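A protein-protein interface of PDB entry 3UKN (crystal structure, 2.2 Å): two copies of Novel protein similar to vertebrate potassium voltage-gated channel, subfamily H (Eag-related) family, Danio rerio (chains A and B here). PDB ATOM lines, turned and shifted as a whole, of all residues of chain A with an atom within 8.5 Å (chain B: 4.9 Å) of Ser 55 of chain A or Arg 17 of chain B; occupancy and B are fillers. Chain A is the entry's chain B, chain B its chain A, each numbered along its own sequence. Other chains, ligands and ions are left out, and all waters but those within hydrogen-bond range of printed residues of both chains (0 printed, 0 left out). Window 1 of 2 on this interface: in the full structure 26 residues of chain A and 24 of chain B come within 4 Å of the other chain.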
ATOM      1  N   ILE A  52     -28.286  -0.789  -7.047  1.00  0.00           N
ATOM      2  CA  ILE A  52     -27.752  -1.259  -5.767  1.00  0.00           C
ATOM      3  C   ILE A  52     -26.541  -0.467  -5.267  1.00  0.00           C
ATOM      4  O   ILE A  52     -25.772   0.107  -6.045  1.00  0.00           O
ATOM      5  CB  ILE A  52     -27.404  -2.771  -5.781  1.00  0.00           C
ATOM      6  CG1 ILE A  52     -26.082  -3.025  -6.500  1.00  0.00           C
ATOM      7  CG2 ILE A  52     -28.532  -3.587  -6.389  1.00  0.00           C
ATOM      8  CD1 ILE A  52     -25.702  -4.501  -6.556  1.00  0.00           C
ATOM      9  N   ASP A  53     -26.389  -0.432  -3.949  1.00  0.00           N
ATOM     10  CA  ASP A  53     -25.260   0.221  -3.307  1.00  0.00           C
ATOM     11  C   ASP A  53     -24.069  -0.716  -3.354  1.00  0.00           C
ATOM     12  O   ASP A  53     -24.117  -1.783  -2.740  1.00  0.00           O
ATOM     13  CB  ASP A  53     -25.622   0.545  -1.855  1.00  0.00           C
ATOM     14  CG  ASP A  53     -24.450   1.102  -1.066  1.00  0.00           C
ATOM     15  OD1 ASP A  53     -23.448   1.501  -1.695  1.00  0.00           O
ATOM     16  OD2 ASP A  53     -24.536   1.147   0.185  1.00  0.00           O
ATOM     17  N   VAL A  54     -23.010  -0.321  -4.070  1.00  0.00           N
ATOM     18  CA  VAL A  54     -21.825  -1.172  -4.240  1.00  0.00           C
ATOM     19  C   VAL A  54     -20.623  -0.720  -3.416  1.00  0.00           C
ATOM     20  O   VAL A  54     -19.542  -1.314  -3.489  1.00  0.00           O
ATOM     21  CB  VAL A  54     -21.385  -1.287  -5.729  1.00  0.00           C
ATOM     22  CG1 VAL A  54     -22.518  -1.833  -6.578  1.00  0.00           C
ATOM     23  CG2 VAL A  54     -20.894   0.052  -6.258  1.00  0.00           C
ATOM     24  N   SER A  55     -20.812   0.332  -2.630  1.00  0.00           N
ATOM     25  CA  SER A  55     -19.748   0.838  -1.770  1.00  0.00           C
ATOM     26  C   SER A  55     -19.473  -0.168  -0.656  1.00  0.00           C
ATOM     27  O   SER A  55     -20.317  -1.011  -0.360  1.00  0.00           O
ATOM     28  CB  SER A  55     -20.139   2.196  -1.168  1.00  0.00           C
ATOM     29  OG  SER A  55     -21.080   2.041  -0.116  1.00  0.00           O
ATOM     30  N   GLU A  56     -18.304  -0.058  -0.030  1.00  0.00           N
ATOM     31  CA  GLU A  56     -17.903  -0.974   1.030  1.00  0.00           C
ATOM     32  C   GLU A  56     -17.141  -0.156   2.061  1.00  0.00           C
ATOM     33  O   GLU A  56     -15.930   0.077   1.915  1.00  0.00           O
ATOM     34  CB  GLU A  56     -17.024  -2.095   0.446  1.00  0.00           C
ATOM     35  CG  GLU A  56     -16.913  -3.381   1.272  1.00  0.00           C
ATOM     36  CD  GLU A  56     -15.983  -4.437   0.637  1.00  0.00           C
ATOM     37  OE1 GLU A  56     -16.136  -4.710  -0.583  1.00  0.00           O
ATOM     38  OE2 GLU A  56     -15.107  -4.998   1.360  1.00  0.00           O
ATOM     39  N   LEU A  57     -17.850   0.283   3.101  1.00  0.00           N
ATOM     40  CA  LEU A  57     -17.298   1.239   4.073  1.00  0.00           C
ATOM     41  C   LEU A  57     -16.224   0.636   4.946  1.00  0.00           C
ATOM     42  O   LEU A  57     -15.413   1.356   5.520  1.00  0.00           O
ATOM     43  CB  LEU A  57     -18.393   1.798   4.988  1.00  0.00           C
ATOM     44  CG  LEU A  57     -19.258   2.981   4.544  1.00  0.00           C
ATOM     45  CD1 LEU A  57     -20.535   3.001   5.373  1.00  0.00           C
ATOM     46  CD2 LEU A  57     -18.505   4.329   4.644  1.00  0.00           C
ATOM     47  N   LEU A  58     -16.218  -0.689   5.050  1.00  0.00           N
ATOM     48  CA  LEU A  58     -15.417  -1.360   6.078  1.00  0.00           C
ATOM     49  C   LEU A  58     -14.211  -2.065   5.492  1.00  0.00           C
ATOM     50  O   LEU A  58     -13.404  -2.639   6.227  1.00  0.00           O
ATOM     51  CB  LEU A  58     -16.275  -2.361   6.854  1.00  0.00           C
ATOM     52  CG  LEU A  58     -17.626  -1.826   7.325  1.00  0.00           C
ATOM     53  CD1 LEU A  58     -18.408  -2.919   7.998  1.00  0.00           C
ATOM     54  CD2 LEU A  58     -17.474  -0.605   8.252  1.00  0.00           C
ATOM     55  N   LYS A  59     -14.096  -2.010   4.168  1.00  0.00           N
ATOM     56  CA  LYS A  59     -13.030  -2.692   3.442  1.00  0.00           C
ATOM     57  C   LYS A  59     -11.609  -2.387   3.929  1.00  0.00           C
ATOM     58  O   LYS A  59     -10.760  -3.278   3.958  1.00  0.00           O
ATOM     59  CB  LYS A  59     -13.119  -2.388   1.948  1.00  0.00           C
ATOM     60  CG  LYS A  59     -11.978  -2.999   1.151  1.00  0.00           C
ATOM     61  CD  LYS A  59     -12.300  -3.050  -0.342  1.00  0.00           C
ATOM     62  CE  LYS A  59     -11.518  -4.160  -1.043  1.00  0.00           C
ATOM     63  NZ  LYS A  59     -12.176  -4.538  -2.326  1.00  0.00           N
ATOM     64  N   LEU A  96     -20.370  -8.554   6.591  1.00  0.00           N
ATOM     65  CA  LEU A  96     -19.937  -7.162   6.479  1.00  0.00           C
ATOM     66  C   LEU A  96     -20.262  -6.483   5.127  1.00  0.00           C
ATOM     67  O   LEU A  96     -20.132  -5.266   5.009  1.00  0.00           O
ATOM     68  CB  LEU A  96     -18.443  -7.038   6.804  1.00  0.00           C
ATOM     69  CG  LEU A  96     -18.010  -7.406   8.226  1.00  0.00           C
ATOM     70  CD1 LEU A  96     -16.493  -7.557   8.329  1.00  0.00           C
ATOM     71  CD2 LEU A  96     -18.534  -6.392   9.237  1.00  0.00           C
ATOM     72  N   ILE A  97     -20.671  -7.257   4.118  1.00  0.00           N
ATOM     73  CA  ILE A  97     -21.005  -6.697   2.801  1.00  0.00           C
ATOM     74  C   ILE A  97     -22.501  -6.834   2.489  1.00  0.00           C
ATOM     75  O   ILE A  97     -22.935  -6.626   1.359  1.00  0.00           O
ATOM     76  CB  ILE A  97     -20.171  -7.329   1.618  1.00  0.00           C
ATOM     77  CG1 ILE A  97     -20.502  -8.825   1.436  1.00  0.00           C
ATOM     78  CG2 ILE A  97     -18.655  -7.077   1.796  1.00  0.00           C
ATOM     79  CD1 ILE A  97     -19.811  -9.499   0.231  1.00  0.00           C
ATOM     80  N   ILE A  98     -23.289  -7.179   3.500  1.00  0.00           N
ATOM     81  CA  ILE A  98     -24.729  -7.313   3.317  1.00  0.00           C
ATOM     82  C   ILE A  98     -25.407  -5.949   3.453  1.00  0.00           C
ATOM     83  O   ILE A  98     -25.121  -5.204   4.380  1.00  0.00           O
ATOM     84  CB  ILE A  98     -25.349  -8.313   4.350  1.00  0.00           C
ATOM     85  CG1 ILE A  98     -24.878  -9.739   4.076  1.00  0.00           C
ATOM     86  CG2 ILE A  98     -26.864  -8.245   4.336  1.00  0.00           C
ATOM     87  CD1 ILE A  98     -25.427 -10.729   5.044  1.00  0.00           C
ATOM     88  N   LYS A  99     -26.311  -5.635   2.534  1.00  0.00           N
ATOM     89  CA  LYS A  99     -27.002  -4.348   2.516  1.00  0.00           C
ATOM     90  C   LYS A  99     -28.485  -4.591   2.662  1.00  0.00           C
ATOM     91  O   LYS A  99     -28.948  -5.729   2.560  1.00  0.00           O
ATOM     92  CB  LYS A  99     -26.797  -3.647   1.169  1.00  0.00           C
ATOM     93  CG  LYS A  99     -25.366  -3.604   0.683  1.00  0.00           C
ATOM     94  CD  LYS A  99     -24.679  -2.375   1.217  1.00  0.00           C
ATOM     95  CE  LYS A  99     -23.274  -2.255   0.649  1.00  0.00           C
ATOM     96  NZ  LYS A  99     -22.598  -1.058   1.224  1.00  0.00           N
ATOM     97  N   TYR A 172     -29.434  -8.039   0.796  1.00  0.00           N
ATOM     98  CA  TYR A 172     -28.796  -8.521  -0.419  1.00  0.00           C
ATOM     99  C   TYR A 172     -27.284  -8.440  -0.334  1.00  0.00           C
ATOM    100  O   TYR A 172     -26.729  -7.709   0.493  1.00  0.00           O
ATOM    101  CB  TYR A 172     -29.317  -7.742  -1.644  1.00  0.00           C
ATOM    102  CG  TYR A 172     -28.915  -6.276  -1.695  1.00  0.00           C
ATOM    103  CD1 TYR A 172     -27.728  -5.874  -2.324  1.00  0.00           C
ATOM    104  CD2 TYR A 172     -29.728  -5.285  -1.131  1.00  0.00           C
ATOM    105  CE1 TYR A 172     -27.358  -4.504  -2.387  1.00  0.00           C
ATOM    106  CE2 TYR A 172     -29.360  -3.914  -1.189  1.00  0.00           C
ATOM    107  CZ  TYR A 172     -28.178  -3.541  -1.809  1.00  0.00           C
ATOM    108  OH  TYR A 172     -27.837  -2.201  -1.860  1.00  0.00           O
ATOM    109  N   SER A 174     -24.055  -8.252  -3.336  1.00  0.00           N
ATOM    110  CA  SER A 174     -23.750  -8.112  -4.749  1.00  0.00           C
ATOM    111  C   SER A 174     -23.036  -9.356  -5.197  1.00  0.00           C
ATOM    112  O   SER A 174     -22.300  -9.977  -4.418  1.00  0.00           O
ATOM    113  CB  SER A 174     -22.831  -6.914  -4.984  1.00  0.00           C
ATOM    114  OG  SER A 174     -21.582  -7.122  -4.344  1.00  0.00           O
ATOM    115  N   LYS A 176     -20.634  -9.370  -7.219  1.00  0.00           N
ATOM    116  CA  LYS A 176     -19.227  -9.001  -7.194  1.00  0.00           C
ATOM    117  C   LYS A 176     -18.635  -9.293  -5.815  1.00  0.00           C
ATOM    118  O   LYS A 176     -17.609  -9.947  -5.708  1.00  0.00           O
ATOM    119  CB  LYS A 176     -19.082  -7.521  -7.531  1.00  0.00           C
ATOM    120  CG  LYS A 176     -17.660  -7.026  -7.765  1.00  0.00           C
ATOM    121  CD  LYS A 176     -17.691  -5.526  -8.064  1.00  0.00           C
ATOM    122  CE  LYS A 176     -16.439  -4.801  -7.592  1.00  0.00           C
ATOM    123  NZ  LYS A 176     -15.242  -5.156  -8.407  1.00  0.00           N
ATOM    124  N   LEU B  13     -17.918  14.000  -0.366  1.00  0.00           N
ATOM    125  CA  LEU B  13     -17.924  12.550  -0.254  1.00  0.00           C
ATOM    126  C   LEU B  13     -17.577  12.194   1.168  1.00  0.00           C
ATOM    127  O   LEU B  13     -18.131  11.255   1.739  1.00  0.00           O
ATOM    128  CB  LEU B  13     -16.915  11.890  -1.213  1.00  0.00           C
ATOM    129  CG  LEU B  13     -17.367  11.699  -2.664  1.00  0.00           C
ATOM    130  CD1 LEU B  13     -16.223  11.205  -3.522  1.00  0.00           C
ATOM    131  CD2 LEU B  13     -18.552  10.755  -2.766  1.00  0.00           C
ATOM    132  N   TYR B  14     -16.652  12.953   1.743  1.00  0.00           N
ATOM    133  CA  TYR B  14     -16.265  12.700   3.120  1.00  0.00           C
ATOM    134  C   TYR B  14     -17.486  12.809   4.033  1.00  0.00           C
ATOM    135  O   TYR B  14     -17.744  11.912   4.838  1.00  0.00           O
ATOM    136  CB  TYR B  14     -15.126  13.615   3.566  1.00  0.00           C
ATOM    137  CG  TYR B  14     -14.804  13.462   5.027  1.00  0.00           C
ATOM    138  CD1 TYR B  14     -14.005  12.411   5.481  1.00  0.00           C
ATOM    139  CD2 TYR B  14     -15.320  14.346   5.963  1.00  0.00           C
ATOM    140  CE1 TYR B  14     -13.725  12.257   6.829  1.00  0.00           C
ATOM    141  CE2 TYR B  14     -15.039  14.204   7.307  1.00  0.00           C
ATOM    142  CZ  TYR B  14     -14.244  13.161   7.741  1.00  0.00           C
ATOM    143  OH  TYR B  14     -13.978  13.033   9.099  1.00  0.00           O
ATOM    144  N   HIS B  15     -18.261  13.880   3.888  1.00  0.00           N
ATOM    145  CA  HIS B  15     -19.419  14.060   4.764  1.00  0.00           C
ATOM    146  C   HIS B  15     -20.491  13.003   4.501  1.00  0.00           C
ATOM    147  O   HIS B  15     -21.051  12.427   5.434  1.00  0.00           O
ATOM    148  CB  HIS B  15     -19.985  15.484   4.671  1.00  0.00           C
ATOM    149  CG  HIS B  15     -19.085  16.522   5.263  1.00  0.00           C
ATOM    150  ND1 HIS B  15     -18.099  17.160   4.536  1.00  0.00           N
ATOM    151  CD2 HIS B  15     -19.000  17.019   6.520  1.00  0.00           C
ATOM    152  CE1 HIS B  15     -17.461  18.012   5.316  1.00  0.00           C
ATOM    153  NE2 HIS B  15     -17.988  17.948   6.527  1.00  0.00           N
ATOM    154  N   THR B  16     -20.748  12.735   3.228  1.00  0.00           N
ATOM    155  CA  THR B  16     -21.678  11.686   2.832  1.00  0.00           C
ATOM    156  C   THR B  16     -21.316  10.343   3.442  1.00  0.00           C
ATOM    157  O   THR B  16     -22.158   9.686   4.047  1.00  0.00           O
ATOM    158  CB  THR B  16     -21.716  11.523   1.302  1.00  0.00           C
ATOM    159  OG1 THR B  16     -22.442  12.617   0.735  1.00  0.00           O
ATOM    160  CG2 THR B  16     -22.399  10.206   0.917  1.00  0.00           C
ATOM    161  N   ARG B  17     -20.060   9.938   3.283  1.00  0.00           N
ATOM    162  CA  ARG B  17     -19.605   8.664   3.824  1.00  0.00           C
ATOM    163  C   ARG B  17     -19.590   8.675   5.353  1.00  0.00           C
ATOM    164  O   ARG B  17     -19.834   7.653   5.991  1.00  0.00           O
ATOM    165  CB  ARG B  17     -18.243   8.272   3.248  1.00  0.00           C
ATOM    166  CG  ARG B  17     -18.321   7.406   1.976  1.00  0.00           C
ATOM    167  CD  ARG B  17     -19.177   8.061   0.917  1.00  0.00           C
ATOM    168  NE  ARG B  17     -18.951   7.541  -0.433  1.00  0.00           N
ATOM    169  CZ  ARG B  17     -19.553   6.469  -0.946  1.00  0.00           C
ATOM    170  NH1 ARG B  17     -20.409   5.767  -0.211  1.00  0.00           N
ATOM    171  NH2 ARG B  17     -19.296   6.096  -2.198  1.00  0.00           N
ATOM    172  N   THR B  18     -19.334   9.833   5.949  1.00  0.00           N
ATOM    173  CA  THR B  18     -19.370   9.917   7.402  1.00  0.00           C
ATOM    174  C   THR B  18     -20.778   9.605   7.899  1.00  0.00           C
ATOM    175  O   THR B  18     -20.961   8.813   8.829  1.00  0.00           O
ATOM    176  CB  THR B  18     -18.901  11.297   7.924  1.00  0.00           C
ATOM    177  OG1 THR B  18     -17.534  11.504   7.547  1.00  0.00           O
ATOM    178  CG2 THR B  18     -19.018  11.361   9.442  1.00  0.00           C
ATOM    179  N   LYS B  19     -21.772  10.211   7.257  1.00  0.00           N
ATOM    180  CA  LYS B  19     -23.155   9.992   7.648  1.00  0.00           C
ATOM    181  C   LYS B  19     -23.511   8.514   7.476  1.00  0.00           C
ATOM    182  O   LYS B  19     -24.137   7.913   8.339  1.00  0.00           O
ATOM    183  CB  LYS B  19     -24.096  10.908   6.853  1.00  0.00           C
ATOM    184  N   ASP B  20     -23.085   7.924   6.368  1.00  0.00           N
ATOM    185  CA  ASP B  20     -23.304   6.506   6.125  1.00  0.00           C
ATOM    186  C   ASP B  20     -22.731   5.613   7.227  1.00  0.00           C
ATOM    187  O   ASP B  20     -23.394   4.705   7.717  1.00  0.00           O
ATOM    188  CB  ASP B  20     -22.708   6.117   4.779  1.00  0.00           C
ATOM    189  CG  ASP B  20     -23.424   6.780   3.628  1.00  0.00           C
ATOM    190  OD1 ASP B  20     -24.599   7.180   3.818  1.00  0.00           O
ATOM    191  OD2 ASP B  20     -22.817   6.905   2.545  1.00  0.00           O
ATOM    192  N   LEU B  21     -21.496   5.881   7.616  1.00  0.00           N
ATOM    193  CA  LEU B  21     -20.874   5.128   8.683  1.00  0.00           C
ATOM    194  C   LEU B  21     -21.664   5.274   9.986  1.00  0.00           C
ATOM    195  O   LEU B  21     -21.932   4.289  10.664  1.00  0.00           O
ATOM    196  CB  LEU B  21     -19.420   5.559   8.862  1.00  0.00           C
ATOM    197  CG  LEU B  21     -18.690   4.690   9.874  1.00  0.00           C
ATOM    198  CD1 LEU B  21     -18.672   3.212   9.401  1.00  0.00           C
ATOM    199  CD2 LEU B  21     -17.284   5.241  10.098  1.00  0.00           C
ATOM    200  N   PHE B  42     -12.014   5.367  10.313  1.00  0.00           N
ATOM    201  CA  PHE B  42     -12.468   6.021   9.092  1.00  0.00           C
ATOM    202  C   PHE B  42     -11.565   7.198   8.684  1.00  0.00           C
ATOM    203  O   PHE B  42     -11.071   7.262   7.563  1.00  0.00           O
ATOM    204  CB  PHE B  42     -13.908   6.497   9.271  1.00  0.00           C
ATOM    205  CG  PHE B  42     -14.587   6.849   7.977  1.00  0.00           C
ATOM    206  CD1 PHE B  42     -14.925   5.854   7.068  1.00  0.00           C
ATOM    207  CD2 PHE B  42     -14.900   8.159   7.671  1.00  0.00           C
ATOM    208  CE1 PHE B  42     -15.563   6.172   5.874  1.00  0.00           C
ATOM    209  CE2 PHE B  42     -15.533   8.477   6.481  1.00  0.00           C
ATOM    210  CZ  PHE B  42     -15.874   7.475   5.587  1.00  0.00           C
ATOM    211  N   TRP B  46      -9.279   7.494   5.493  1.00  0.00           N
ATOM    212  CA  TRP B  46     -10.097   8.159   4.468  1.00  0.00           C
ATOM    213  C   TRP B  46      -9.277   8.783   3.335  1.00  0.00           C
ATOM    214  O   TRP B  46      -8.238   9.409   3.557  1.00  0.00           O
ATOM    215  CB  TRP B  46     -11.027   9.221   5.074  1.00  0.00           C
ATOM    216  CG  TRP B  46     -11.675  10.060   4.003  1.00  0.00           C
ATOM    217  CD1 TRP B  46     -11.312  11.324   3.617  1.00  0.00           C
ATOM    218  CD2 TRP B  46     -12.765   9.675   3.140  1.00  0.00           C
ATOM    219  NE1 TRP B  46     -12.117  11.751   2.583  1.00  0.00           N
ATOM    220  CE2 TRP B  46     -13.010  10.766   2.277  1.00  0.00           C
ATOM    221  CE3 TRP B  46     -13.547   8.524   3.022  1.00  0.00           C
ATOM    222  CZ2 TRP B  46     -14.026  10.733   1.308  1.00  0.00           C
ATOM    223  CZ3 TRP B  46     -14.546   8.498   2.061  1.00  0.00           C
ATOM    224  CH2 TRP B  46     -14.775   9.597   1.212  1.00  0.00           C
ATOM    225  N   GLY B  51     -13.370   6.539  -1.527  1.00  0.00           N
ATOM    226  CA  GLY B  51     -14.791   6.691  -1.254  1.00  0.00           C
ATOM    227  C   GLY B  51     -15.605   7.138  -2.452  1.00  0.00           C
ATOM    228  O   GLY B  51     -16.747   7.536  -2.303  1.00  0.00           O
ATOM    229  N   ILE B  52     -15.035   7.084  -3.649  1.00  0.00           N
ATOM    230  CA  ILE B  52     -15.756   7.667  -4.788  1.00  0.00           C
ATOM    231  C   ILE B  52     -17.113   7.029  -5.131  1.00  0.00           C
ATOM    232  O   ILE B  52     -17.313   5.834  -4.996  1.00  0.00           O
ATOM    233  CB  ILE B  52     -14.897   7.759  -6.063  1.00  0.00           C
ATOM    234  CG1 ILE B  52     -14.337   6.391  -6.442  1.00  0.00           C
ATOM    235  CG2 ILE B  52     -13.801   8.801  -5.887  1.00  0.00           C
ATOM    236  CD1 ILE B  52     -14.186   6.214  -7.961  1.00  0.00           C
ATOM    237  N   ASP B  53     -18.039   7.864  -5.582  1.00  0.00           N
ATOM    238  CA  ASP B  53     -19.346   7.418  -6.053  1.00  0.00           C
ATOM    239  C   ASP B  53     -19.206   6.778  -7.438  1.00  0.00           C
ATOM    240  O   ASP B  53     -18.837   7.453  -8.392  1.00  0.00           O
ATOM    241  CB  ASP B  53     -20.298   8.615  -6.118  1.00  0.00           C
ATOM    242  CG  ASP B  53     -21.646   8.258  -6.717  1.00  0.00           C
ATOM    243  OD1 ASP B  53     -22.168   7.167  -6.400  1.00  0.00           O
ATOM    244  OD2 ASP B  53     -22.184   9.067  -7.504  1.00  0.00           O
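The guanidinium group (NH1) of Arg 17 of chain B is in salt-bridge range of the side-chain carboxylate (OD2) of Asp 20 of chain B (3.8 Å). The guanidinium group (NE) of Arg 17 of chain B sits at hydrogen-bond distance from the backbone carbonyl oxygen (O) of Gly 51 of chain B (2.9 Å). The guanidinium group of Arg 17 of chain B is in hydrogen-bond range of the backbone carbonyl oxygen of Ile 52 of chain B (3.4 Å). OG of Ser 55 of chain A is in hydrogen-bond range of OD1 of Asp 53 of chain A (2.9 Å). The side-chain amino group of Lys 99 of chain A lies within hydrogen-bond range of the backbone carbonyl oxygen of Ser 55 of chain A (2.8 Å).
Arg 17 of chain B touches Ser 55 of chain A (NH1 to CB, 3.7 Å). Arg 17 of chain B touches Leu 57 of chain A. CB of Asp 20 of chain B touches CD1 of Leu 57 of chain A, at 3.8 Å. Leu 57 of chain A touches Leu 21 of chain B. Phe 42 of chain B touches Leu 57 of chain A.
Printed residues of chain B within 4 Å of Ser 55 of chain A: Arg 17. Of the printed residues of chain B, Leu 57 of chain A touches Arg 17 (3.8 Å), Asp 20 (3.8 Å), Leu 21 (3.8 Å) and Phe 42 (3.7 Å). No residue of chain A comes within 4 Å of Thr 16 of chain B. Arg 17 of chain B touches two residues of chain A. Of the printed residues of chain A, Asp 20 of chain B touches Leu 57 (3.8 Å). Of the printed residues of chain A, Leu 21 of chain B touches Leu 57 (3.8 Å). Of the printed residues of chain A, Phe 42 of chain B touches Leu 57 (3.7 Å). The nearest printed residue of chain B that does not touch Ser 55 of chain A is Asp 20 of chain B (5.8 Å). The nearest residue of chain A that does not touch Arg 17 of chain B is Asp 53 of chain A (5.4 Å). The nearest printed residue of chain B that does not touch Leu 57 of chain A is Thr 18 of chain B (5.7 Å).
Printed residues of chain A that touch a printed residue of chain B: Ser 55 and Leu 57. Of the 14 printed residues of chain B, 4 touch a printed residue of chain A. Along chain B the printed residues that touch a printed residue of chain A span positions 17 to 42. Among the printed residues, 5 pairs touch across the chains. Among the printed residues, no Asp or Glu carboxylate lies within 4 Å of a Lys or Arg side-chain nitrogen of the other chain.
2 positions are printed for both chains.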
